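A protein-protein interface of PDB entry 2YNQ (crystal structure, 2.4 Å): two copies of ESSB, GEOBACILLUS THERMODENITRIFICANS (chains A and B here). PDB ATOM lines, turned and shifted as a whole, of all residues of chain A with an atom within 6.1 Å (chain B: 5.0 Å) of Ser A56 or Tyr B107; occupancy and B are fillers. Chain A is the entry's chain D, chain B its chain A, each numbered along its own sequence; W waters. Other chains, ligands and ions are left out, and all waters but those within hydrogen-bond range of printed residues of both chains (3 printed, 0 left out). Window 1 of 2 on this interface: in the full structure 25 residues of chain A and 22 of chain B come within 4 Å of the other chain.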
ATOM      1  N   THR A  54      22.955  24.515 -20.497  1.00  0.00           N
ATOM      2  CA  THR A  54      24.228  24.306 -21.171  1.00  0.00           C
ATOM      3  C   THR A  54      24.549  22.815 -21.337  1.00  0.00           C
ATOM      4  O   THR A  54      25.666  22.453 -21.698  1.00  0.00           O
ATOM      5  CB  THR A  54      25.373  25.001 -20.399  1.00  0.00           C
ATOM      6  OG1 THR A  54      25.418  24.506 -19.053  1.00  0.00           O
ATOM      7  CG2 THR A  54      25.153  26.487 -20.349  1.00  0.00           C
ATOM      8  N   GLU A  55      23.590  21.945 -21.047  1.00  0.00           N
ATOM      9  CA  GLU A  55      23.778  20.508 -21.277  1.00  0.00           C
ATOM     10  C   GLU A  55      23.671  20.218 -22.784  1.00  0.00           C
ATOM     11  O   GLU A  55      22.712  20.625 -23.430  1.00  0.00           O
ATOM     12  CB  GLU A  55      22.747  19.701 -20.477  1.00  0.00           C
ATOM     13  CG  GLU A  55      22.884  18.197 -20.578  1.00  0.00           C
ATOM     14  CD  GLU A  55      24.098  17.639 -19.843  1.00  0.00           C
ATOM     15  OE1 GLU A  55      24.786  18.382 -19.112  1.00  0.00           O
ATOM     16  OE2 GLU A  55      24.378  16.436 -20.007  1.00  0.00           O
ATOM     17  N   SER A  56      24.666  19.547 -23.343  1.00  0.00           N
ATOM     18  CA  SER A  56      24.642  19.164 -24.769  1.00  0.00           C
ATOM     19  C   SER A  56      23.634  18.082 -25.045  1.00  0.00           C
ATOM     20  O   SER A  56      23.993  16.929 -25.095  1.00  0.00           O
ATOM     21  CB  SER A  56      25.988  18.602 -25.194  1.00  0.00           C
ATOM     22  OG  SER A  56      26.981  19.585 -25.044  1.00  0.00           O
ATOM     23  N   LEU A  57      22.383  18.460 -25.225  1.00  0.00           N
ATOM     24  CA  LEU A  57      21.328  17.533 -25.573  1.00  0.00           C
ATOM     25  C   LEU A  57      20.967  17.736 -27.027  1.00  0.00           C
ATOM     26  O   LEU A  57      20.856  18.870 -27.486  1.00  0.00           O
ATOM     27  CB  LEU A  57      20.089  17.789 -24.706  1.00  0.00           C
ATOM     28  CG  LEU A  57      20.200  17.617 -23.196  1.00  0.00           C
ATOM     29  CD1 LEU A  57      19.123  18.400 -22.501  1.00  0.00           C
ATOM     30  CD2 LEU A  57      20.085  16.161 -22.815  1.00  0.00           C
ATOM     31  N   THR A  58      20.778  16.646 -27.762  1.00  0.00           N
ATOM     32  CA  THR A  58      20.170  16.749 -29.092  1.00  0.00           C
ATOM     33  C   THR A  58      18.696  17.054 -28.867  1.00  0.00           C
ATOM     34  O   THR A  58      18.167  16.883 -27.751  1.00  0.00           O
ATOM     35  CB  THR A  58      20.235  15.431 -29.864  1.00  0.00           C
ATOM     36  OG1 THR A  58      19.489  14.446 -29.142  1.00  0.00           O
ATOM     37  CG2 THR A  58      21.678  14.962 -30.047  1.00  0.00           C
ATOM     38  N   GLU A  59      18.035  17.481 -29.929  1.00  0.00           N
ATOM     39  CA  GLU A  59      16.610  17.714 -29.916  1.00  0.00           C
ATOM     40  C   GLU A  59      15.829  16.481 -29.409  1.00  0.00           C
ATOM     41  O   GLU A  59      14.884  16.621 -28.625  1.00  0.00           O
ATOM     42  CB  GLU A  59      16.162  18.102 -31.331  1.00  0.00           C
ATOM     43  CG  GLU A  59      14.979  19.032 -31.382  1.00  0.00           C
ATOM     44  CD  GLU A  59      15.111  20.183 -30.408  1.00  0.00           C
ATOM     45  OE1 GLU A  59      16.048  21.016 -30.557  1.00  0.00           O
ATOM     46  OE2 GLU A  59      14.269  20.240 -29.482  1.00  0.00           O
ATOM     47  N   GLN A  61      16.977  14.008 -27.367  1.00  0.00           N
ATOM     48  CA  GLN A  61      17.247  13.884 -25.934  1.00  0.00           C
ATOM     49  C   GLN A  61      16.366  14.862 -25.174  1.00  0.00           C
ATOM     50  O   GLN A  61      15.689  14.496 -24.209  1.00  0.00           O
ATOM     51  CB  GLN A  61      18.729  14.140 -25.620  1.00  0.00           C
ATOM     52  CG  GLN A  61      19.649  13.001 -26.020  1.00  0.00           C
ATOM     53  CD  GLN A  61      21.131  13.289 -25.819  1.00  0.00           C
ATOM     54  OE1 GLN A  61      21.698  14.239 -26.368  1.00  0.00           O
ATOM     55  NE2 GLN A  61      21.774  12.439 -25.045  1.00  0.00           N
ATOM     56  N   ARG A  62      16.378  16.099 -25.651  1.00  0.00           N
ATOM     57  CA  ARG A  62      15.592  17.186 -25.116  1.00  0.00           C
ATOM     58  C   ARG A  62      14.115  16.854 -24.981  1.00  0.00           C
ATOM     59  O   ARG A  62      13.513  17.130 -23.952  1.00  0.00           O
ATOM     60  CB  ARG A  62      15.738  18.364 -26.055  1.00  0.00           C
ATOM     61  CG  ARG A  62      15.610  19.702 -25.431  1.00  0.00           C
ATOM     62  CD  ARG A  62      15.875  20.722 -26.529  1.00  0.00           C
ATOM     63  NE  ARG A  62      17.310  20.835 -26.795  1.00  0.00           N
ATOM     64  CZ  ARG A  62      18.106  21.676 -26.147  1.00  0.00           C
ATOM     65  NH1 ARG A  62      17.606  22.472 -25.220  1.00  0.00           N
ATOM     66  NH2 ARG A  62      19.394  21.723 -26.433  1.00  0.00           N
ATOM     67  N   TYR A 107      19.149   8.534 -18.849  1.00  0.00           N
ATOM     68  CA  TYR A 107      20.131   9.562 -19.190  1.00  0.00           C
ATOM     69  C   TYR A 107      21.367   9.500 -18.283  1.00  0.00           C
ATOM     70  O   TYR A 107      22.512   9.634 -18.746  1.00  0.00           O
ATOM     71  CB  TYR A 107      19.502  10.939 -19.150  1.00  0.00           C
ATOM     72  CG  TYR A 107      20.403  11.982 -19.719  1.00  0.00           C
ATOM     73  CD1 TYR A 107      20.563  12.105 -21.103  1.00  0.00           C
ATOM     74  CD2 TYR A 107      21.107  12.844 -18.887  1.00  0.00           C
ATOM     75  CE1 TYR A 107      21.397  13.060 -21.641  1.00  0.00           C
ATOM     76  CE2 TYR A 107      21.941  13.822 -19.413  1.00  0.00           C
ATOM     77  CZ  TYR A 107      22.088  13.919 -20.782  1.00  0.00           C
ATOM     78  OH  TYR A 107      22.941  14.857 -21.305  1.00  0.00           O
ATOM     79  N   GLU B  55      27.949   8.032 -30.651  1.00  0.00           N
ATOM     80  CA  GLU B  55      27.572   9.101 -29.746  1.00  0.00           C
ATOM     81  C   GLU B  55      26.900   8.542 -28.481  1.00  0.00           C
ATOM     82  O   GLU B  55      26.435   7.389 -28.450  1.00  0.00           O
ATOM     83  CB  GLU B  55      26.614  10.065 -30.439  1.00  0.00           C
ATOM     84  CG  GLU B  55      27.277  11.103 -31.294  1.00  0.00           C
ATOM     85  CD  GLU B  55      28.180  12.040 -30.509  1.00  0.00           C
ATOM     86  OE1 GLU B  55      27.803  12.477 -29.400  1.00  0.00           O
ATOM     87  OE2 GLU B  55      29.285  12.339 -31.014  1.00  0.00           O
ATOM     88  N   TYR B  80      28.876  17.908 -41.021  1.00  0.00           N
ATOM     89  CA  TYR B  80      28.407  18.353 -39.714  1.00  0.00           C
ATOM     90  C   TYR B  80      28.695  17.306 -38.653  1.00  0.00           C
ATOM     91  O   TYR B  80      29.377  17.586 -37.663  1.00  0.00           O
ATOM     92  CB  TYR B  80      26.910  18.678 -39.751  1.00  0.00           C
ATOM     93  CG  TYR B  80      26.340  19.057 -38.393  1.00  0.00           C
ATOM     94  CD1 TYR B  80      26.379  20.384 -37.943  1.00  0.00           C
ATOM     95  CD2 TYR B  80      25.770  18.085 -37.553  1.00  0.00           C
ATOM     96  CE1 TYR B  80      25.856  20.732 -36.684  1.00  0.00           C
ATOM     97  CE2 TYR B  80      25.252  18.419 -36.309  1.00  0.00           C
ATOM     98  CZ  TYR B  80      25.302  19.741 -35.878  1.00  0.00           C
ATOM     99  OH  TYR B  80      24.797  20.078 -34.657  1.00  0.00           O
ATOM    100  N   TRP B  81      28.202  16.091 -38.880  1.00  0.00           N
ATOM    101  CA  TRP B  81      28.338  15.021 -37.903  1.00  0.00           C
ATOM    102  C   TRP B  81      29.765  14.533 -37.710  1.00  0.00           C
ATOM    103  O   TRP B  81      30.127  14.062 -36.619  1.00  0.00           O
ATOM    104  CB  TRP B  81      27.397  13.860 -38.207  1.00  0.00           C
ATOM    105  CG  TRP B  81      26.005  14.207 -37.835  1.00  0.00           C
ATOM    106  CD1 TRP B  81      24.956  14.464 -38.688  1.00  0.00           C
ATOM    107  CD2 TRP B  81      25.496  14.386 -36.508  1.00  0.00           C
ATOM    108  NE1 TRP B  81      23.823  14.763 -37.965  1.00  0.00           N
ATOM    109  CE2 TRP B  81      24.127  14.726 -36.628  1.00  0.00           C
ATOM    110  CE3 TRP B  81      26.060  14.280 -35.231  1.00  0.00           C
ATOM    111  CZ2 TRP B  81      23.317  14.975 -35.518  1.00  0.00           C
ATOM    112  CZ3 TRP B  81      25.258  14.522 -34.123  1.00  0.00           C
ATOM    113  CH2 TRP B  81      23.895  14.862 -34.273  1.00  0.00           C
ATOM    114  N   ILE B  84      31.259  17.328 -35.399  1.00  0.00           N
ATOM    115  CA  ILE B  84      30.795  17.007 -34.056  1.00  0.00           C
ATOM    116  C   ILE B  84      31.597  15.845 -33.503  1.00  0.00           C
ATOM    117  O   ILE B  84      32.206  15.970 -32.449  1.00  0.00           O
ATOM    118  CB  ILE B  84      29.288  16.674 -34.014  1.00  0.00           C
ATOM    119  CG1 ILE B  84      28.450  17.931 -34.296  1.00  0.00           C
ATOM    120  CG2 ILE B  84      28.906  15.992 -32.701  1.00  0.00           C
ATOM    121  CD1 ILE B  84      28.592  19.051 -33.247  1.00  0.00           C
ATOM    122  N   ARG B 102      18.041  25.162 -37.456  1.00  0.00           N
ATOM    123  CA  ARG B 102      18.035  25.630 -36.064  1.00  0.00           C
ATOM    124  C   ARG B 102      18.568  24.602 -35.078  1.00  0.00           C
ATOM    125  O   ARG B 102      19.446  24.898 -34.266  1.00  0.00           O
ATOM    126  CB  ARG B 102      16.613  26.039 -35.670  1.00  0.00           C
ATOM    127  CG  ARG B 102      16.407  26.239 -34.191  1.00  0.00           C
ATOM    128  CD  ARG B 102      15.375  27.305 -33.962  1.00  0.00           C
ATOM    129  NE  ARG B 102      15.679  28.485 -34.763  1.00  0.00           N
ATOM    130  CZ  ARG B 102      15.338  29.723 -34.431  1.00  0.00           C
ATOM    131  NH1 ARG B 102      14.683  29.949 -33.300  1.00  0.00           N
ATOM    132  NH2 ARG B 102      15.661  30.735 -35.226  1.00  0.00           N
ATOM    133  N   ASP B 103      18.029  23.392 -35.170  1.00  0.00           N
ATOM    134  CA  ASP B 103      18.396  22.287 -34.284  1.00  0.00           C
ATOM    135  C   ASP B 103      19.889  21.956 -34.331  1.00  0.00           C
ATOM    136  O   ASP B 103      20.492  21.664 -33.297  1.00  0.00           O
ATOM    137  CB  ASP B 103      17.547  21.039 -34.580  1.00  0.00           C
ATOM    138  CG  ASP B 103      16.053  21.234 -34.241  1.00  0.00           C
ATOM    139  OD1 ASP B 103      15.709  22.201 -33.506  1.00  0.00           O
ATOM    140  OD2 ASP B 103      15.208  20.416 -34.704  1.00  0.00           O
ATOM    141  N   LEU B 104      20.495  22.037 -35.511  1.00  0.00           N
ATOM    142  CA  LEU B 104      21.919  21.711 -35.635  1.00  0.00           C
ATOM    143  C   LEU B 104      22.785  22.865 -35.163  1.00  0.00           C
ATOM    144  O   LEU B 104      23.887  22.647 -34.661  1.00  0.00           O
ATOM    145  CB  LEU B 104      22.302  21.295 -37.067  1.00  0.00           C
ATOM    146  CG  LEU B 104      21.547  20.162 -37.794  1.00  0.00           C
ATOM    147  CD1 LEU B 104      22.164  19.899 -39.172  1.00  0.00           C
ATOM    148  CD2 LEU B 104      21.501  18.869 -37.030  1.00  0.00           C
ATOM    149  N   ILE B 105      22.285  24.088 -35.329  1.00  0.00           N
ATOM    150  CA  ILE B 105      22.964  25.277 -34.785  1.00  0.00           C
ATOM    151  C   ILE B 105      23.010  25.212 -33.252  1.00  0.00           C
ATOM    152  O   ILE B 105      24.088  25.324 -32.639  1.00  0.00           O
ATOM    153  CB  ILE B 105      22.311  26.613 -35.262  1.00  0.00           C
ATOM    154  CG1 ILE B 105      22.446  26.757 -36.786  1.00  0.00           C
ATOM    155  CG2 ILE B 105      22.932  27.816 -34.532  1.00  0.00           C
ATOM    156  CD1 ILE B 105      21.660  27.924 -37.392  1.00  0.00           C
ATOM    157  N   VAL B 106      21.848  24.983 -32.648  1.00  0.00           N
ATOM    158  CA  VAL B 106      21.756  24.893 -31.185  1.00  0.00           C
ATOM    159  C   VAL B 106      22.655  23.794 -30.616  1.00  0.00           C
ATOM    160  O   VAL B 106      23.416  24.052 -29.685  1.00  0.00           O
ATOM    161  CB  VAL B 106      20.293  24.753 -30.690  1.00  0.00           C
ATOM    162  CG1 VAL B 106      20.253  24.537 -29.192  1.00  0.00           C
ATOM    163  CG2 VAL B 106      19.492  26.012 -31.063  1.00  0.00           C
ATOM    164  N   TYR B 107      22.617  22.597 -31.206  1.00  0.00           N
ATOM    165  CA  TYR B 107      23.440  21.489 -30.720  1.00  0.00           C
ATOM    166  C   TYR B 107      24.925  21.788 -30.892  1.00  0.00           C
ATOM    167  O   TYR B 107      25.735  21.534 -30.002  1.00  0.00           O
ATOM    168  CB  TYR B 107      23.050  20.153 -31.385  1.00  0.00           C
ATOM    169  CG  TYR B 107      23.774  18.938 -30.815  1.00  0.00           C
ATOM    170  CD1 TYR B 107      23.558  18.529 -29.484  1.00  0.00           C
ATOM    171  CD2 TYR B 107      24.686  18.211 -31.589  1.00  0.00           C
ATOM    172  CE1 TYR B 107      24.220  17.414 -28.939  1.00  0.00           C
ATOM    173  CE2 TYR B 107      25.351  17.076 -31.059  1.00  0.00           C
ATOM    174  CZ  TYR B 107      25.110  16.685 -29.741  1.00  0.00           C
ATOM    175  OH  TYR B 107      25.772  15.598 -29.200  1.00  0.00           O
ATOM    176  N   ALA B 108      25.279  22.359 -32.025  1.00  0.00           N
ATOM    177  CA  ALA B 108      26.659  22.759 -32.270  1.00  0.00           C
ATOM    178  C   ALA B 108      27.146  23.870 -31.330  1.00  0.00           C
ATOM    179  O   ALA B 108      28.287  23.838 -30.867  1.00  0.00           O
ATOM    180  CB  ALA B 108      26.824  23.180 -33.730  1.00  0.00           C
ATOM    181  N   LEU B 109      26.295  24.852 -31.053  1.00  0.00           N
ATOM    182  CA  LEU B 109      26.650  25.901 -30.067  1.00  0.00           C
ATOM    183  C   LEU B 109      27.006  25.286 -28.727  1.00  0.00           C
ATOM    184  O   LEU B 109      28.039  25.597 -28.125  1.00  0.00           O
ATOM    185  CB  LEU B 109      25.486  26.841 -29.835  1.00  0.00           C
ATOM    186  CG  LEU B 109      25.416  28.169 -30.541  1.00  0.00           C
ATOM    187  CD1 LEU B 109      24.137  28.812 -30.040  1.00  0.00           C
ATOM    188  CD2 LEU B 109      26.636  29.013 -30.201  1.00  0.00           C
ATOM    189  N   LEU B 110      26.134  24.390 -28.280  1.00  0.00           N
ATOM    190  CA  LEU B 110      26.330  23.693 -27.020  1.00  0.00           C
ATOM    191  C   LEU B 110      27.630  22.924 -26.999  1.00  0.00           C
ATOM    192  O   LEU B 110      28.346  22.970 -26.016  1.00  0.00           O
ATOM    193  CB  LEU B 110      25.146  22.777 -26.722  1.00  0.00           C
ATOM    194  CG  LEU B 110      23.882  23.549 -26.360  1.00  0.00           C
ATOM    195  CD1 LEU B 110      22.640  22.721 -26.596  1.00  0.00           C
ATOM    196  CD2 LEU B 110      23.960  24.056 -24.933  1.00  0.00           C
ATOM    197  N   LYS B 111      27.952  22.227 -28.087  1.00  0.00           N
ATOM    198  CA  LYS B 111      29.220  21.504 -28.152  1.00  0.00           C
ATOM    199  C   LYS B 111      30.414  22.477 -28.260  1.00  0.00           C
ATOM    200  O   LYS B 111      31.468  22.255 -27.651  1.00  0.00           O
ATOM    201  CB  LYS B 111      29.177  20.450 -29.274  1.00  0.00           C
ATOM    202  CG  LYS B 111      28.520  19.100 -28.846  1.00  0.00           C
ATOM    203  CD  LYS B 111      29.577  18.179 -28.160  1.00  0.00           C
ATOM    204  CE  LYS B 111      29.020  16.836 -27.684  1.00  0.00           C
ATOM    205  NZ  LYS B 111      28.763  15.816 -28.775  1.00  0.00           N
ATOM    206  N   GLU B 114      31.483  23.936 -25.024  1.00  0.00           N
ATOM    207  CA  GLU B 114      32.384  23.001 -24.354  1.00  0.00           C
ATOM    208  C   GLU B 114      33.814  23.053 -24.877  1.00  0.00           C
ATOM    209  O   GLU B 114      34.749  22.828 -24.118  1.00  0.00           O
ATOM    210  CB  GLU B 114      31.839  21.560 -24.451  1.00  0.00           C
ATOM    211  CG  GLU B 114      30.680  21.289 -23.507  1.00  0.00           C
ATOM    212  CD  GLU B 114      29.935  19.968 -23.770  1.00  0.00           C
ATOM    213  OE1 GLU B 114      30.429  19.124 -24.548  1.00  0.00           O
ATOM    214  OE2 GLU B 114      28.847  19.772 -23.168  1.00  0.00           O
HETATM  215  O   HOH W   1      27.012  18.668 -21.524  1.00  0.00           O
HETATM  216  O   HOH W   2      27.447  23.596 -23.376  1.00  0.00           O
HETATM  217  O   HOH W   3      27.977  21.554 -20.768  1.00  0.00           O
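2 positions are printed for both chains. Of the 9 pairs that touch across the chains among the printed residues, none has its exchanged pair printed and touching as well.
Water W3 lies within hydrogen-bond range of the backbone carbonyl oxygen of Thr A54 and the side-chain carboxylate of Glu B114. Water W1 lies within hydrogen-bond range of the side-chain carboxylate of Glu B114, the backbone NH of Ser A56 and the side-chain carboxylate of Glu A55. Water W2 lies within hydrogen-bond range of O of Thr A54 (2.7 Å) and O of Leu B110 (2.9 Å).
Hydrophobic or aromatic side chains of chain B that line the printed part of chain A: Tyr B107 and Leu B110. Of the 9 printed residues of chain A, 7 touch a printed residue of chain B. Among the printed residues, 9 pairs touch across the chains.
Of the printed residues of chain B, Thr A54 touches Leu B110. Ser A56 touches three residues of chain B. Printed residues of chain B within 4 Å of Leu A57: Tyr B107 (3.4 Å). Of the printed residues of chain B, Thr A58 touches Tyr B107. Of the printed residues of chain B, Glu A59 touches Asp B103 (3.2 Å). Tyr B107 touches three residues of chain A. Printed residues of chain A within 4 Å of Leu B110: Thr A54 (3.8 Å), Glu A55 (3.8 Å), Ser A56 (3.8 Å) and Arg A62 (3.4 Å). The nearest residue of chain A that does not touch Tyr B107 is Gln A61 (4.8 Å). The nearest printed residue of chain A that does not touch Leu B110 is Leu A57 (4.3 Å).
OE1 of Glu A59 lies close to OD1 of Asp B103 (3.2 Å). The side-chain carboxylate of Glu B114 lies within hydrogen-bond range of the side-chain hydroxyl of Ser A56 (2.7 Å).
NH2 of Arg A62 is in hydrogen-bond range of O of Leu A57 (3.4 Å). OH of Tyr B107 sits at hydrogen-bond distance from NZ of Lys B111 (3.0 Å). NE of Arg A62 is in salt-bridge range of OE1 of Glu A59. The side-chain carboxylate (OE2) of Glu A55 sits at hydrogen-bond distance from the side-chain hydroxyl (OH) of Tyr A107 (2.5 Å). N of Thr A58 sits at hydrogen-bond distance from OE1 of Gln A61 (2.9 Å).
Among the printed residues, merely in contact across the chains: Thr A54 with Leu B110 (3.8 Å), Glu A55 with Leu B110 (3.8 Å), Ser A56 with Tyr B107 (3.9 Å), Ser A56 with Leu B110 (3.8 Å), Leu A57 with Tyr B107 (3.4 Å), Thr A58 with Tyr B107 (3.7 Å) and Arg A62 with Leu B110 (3.4 Å).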
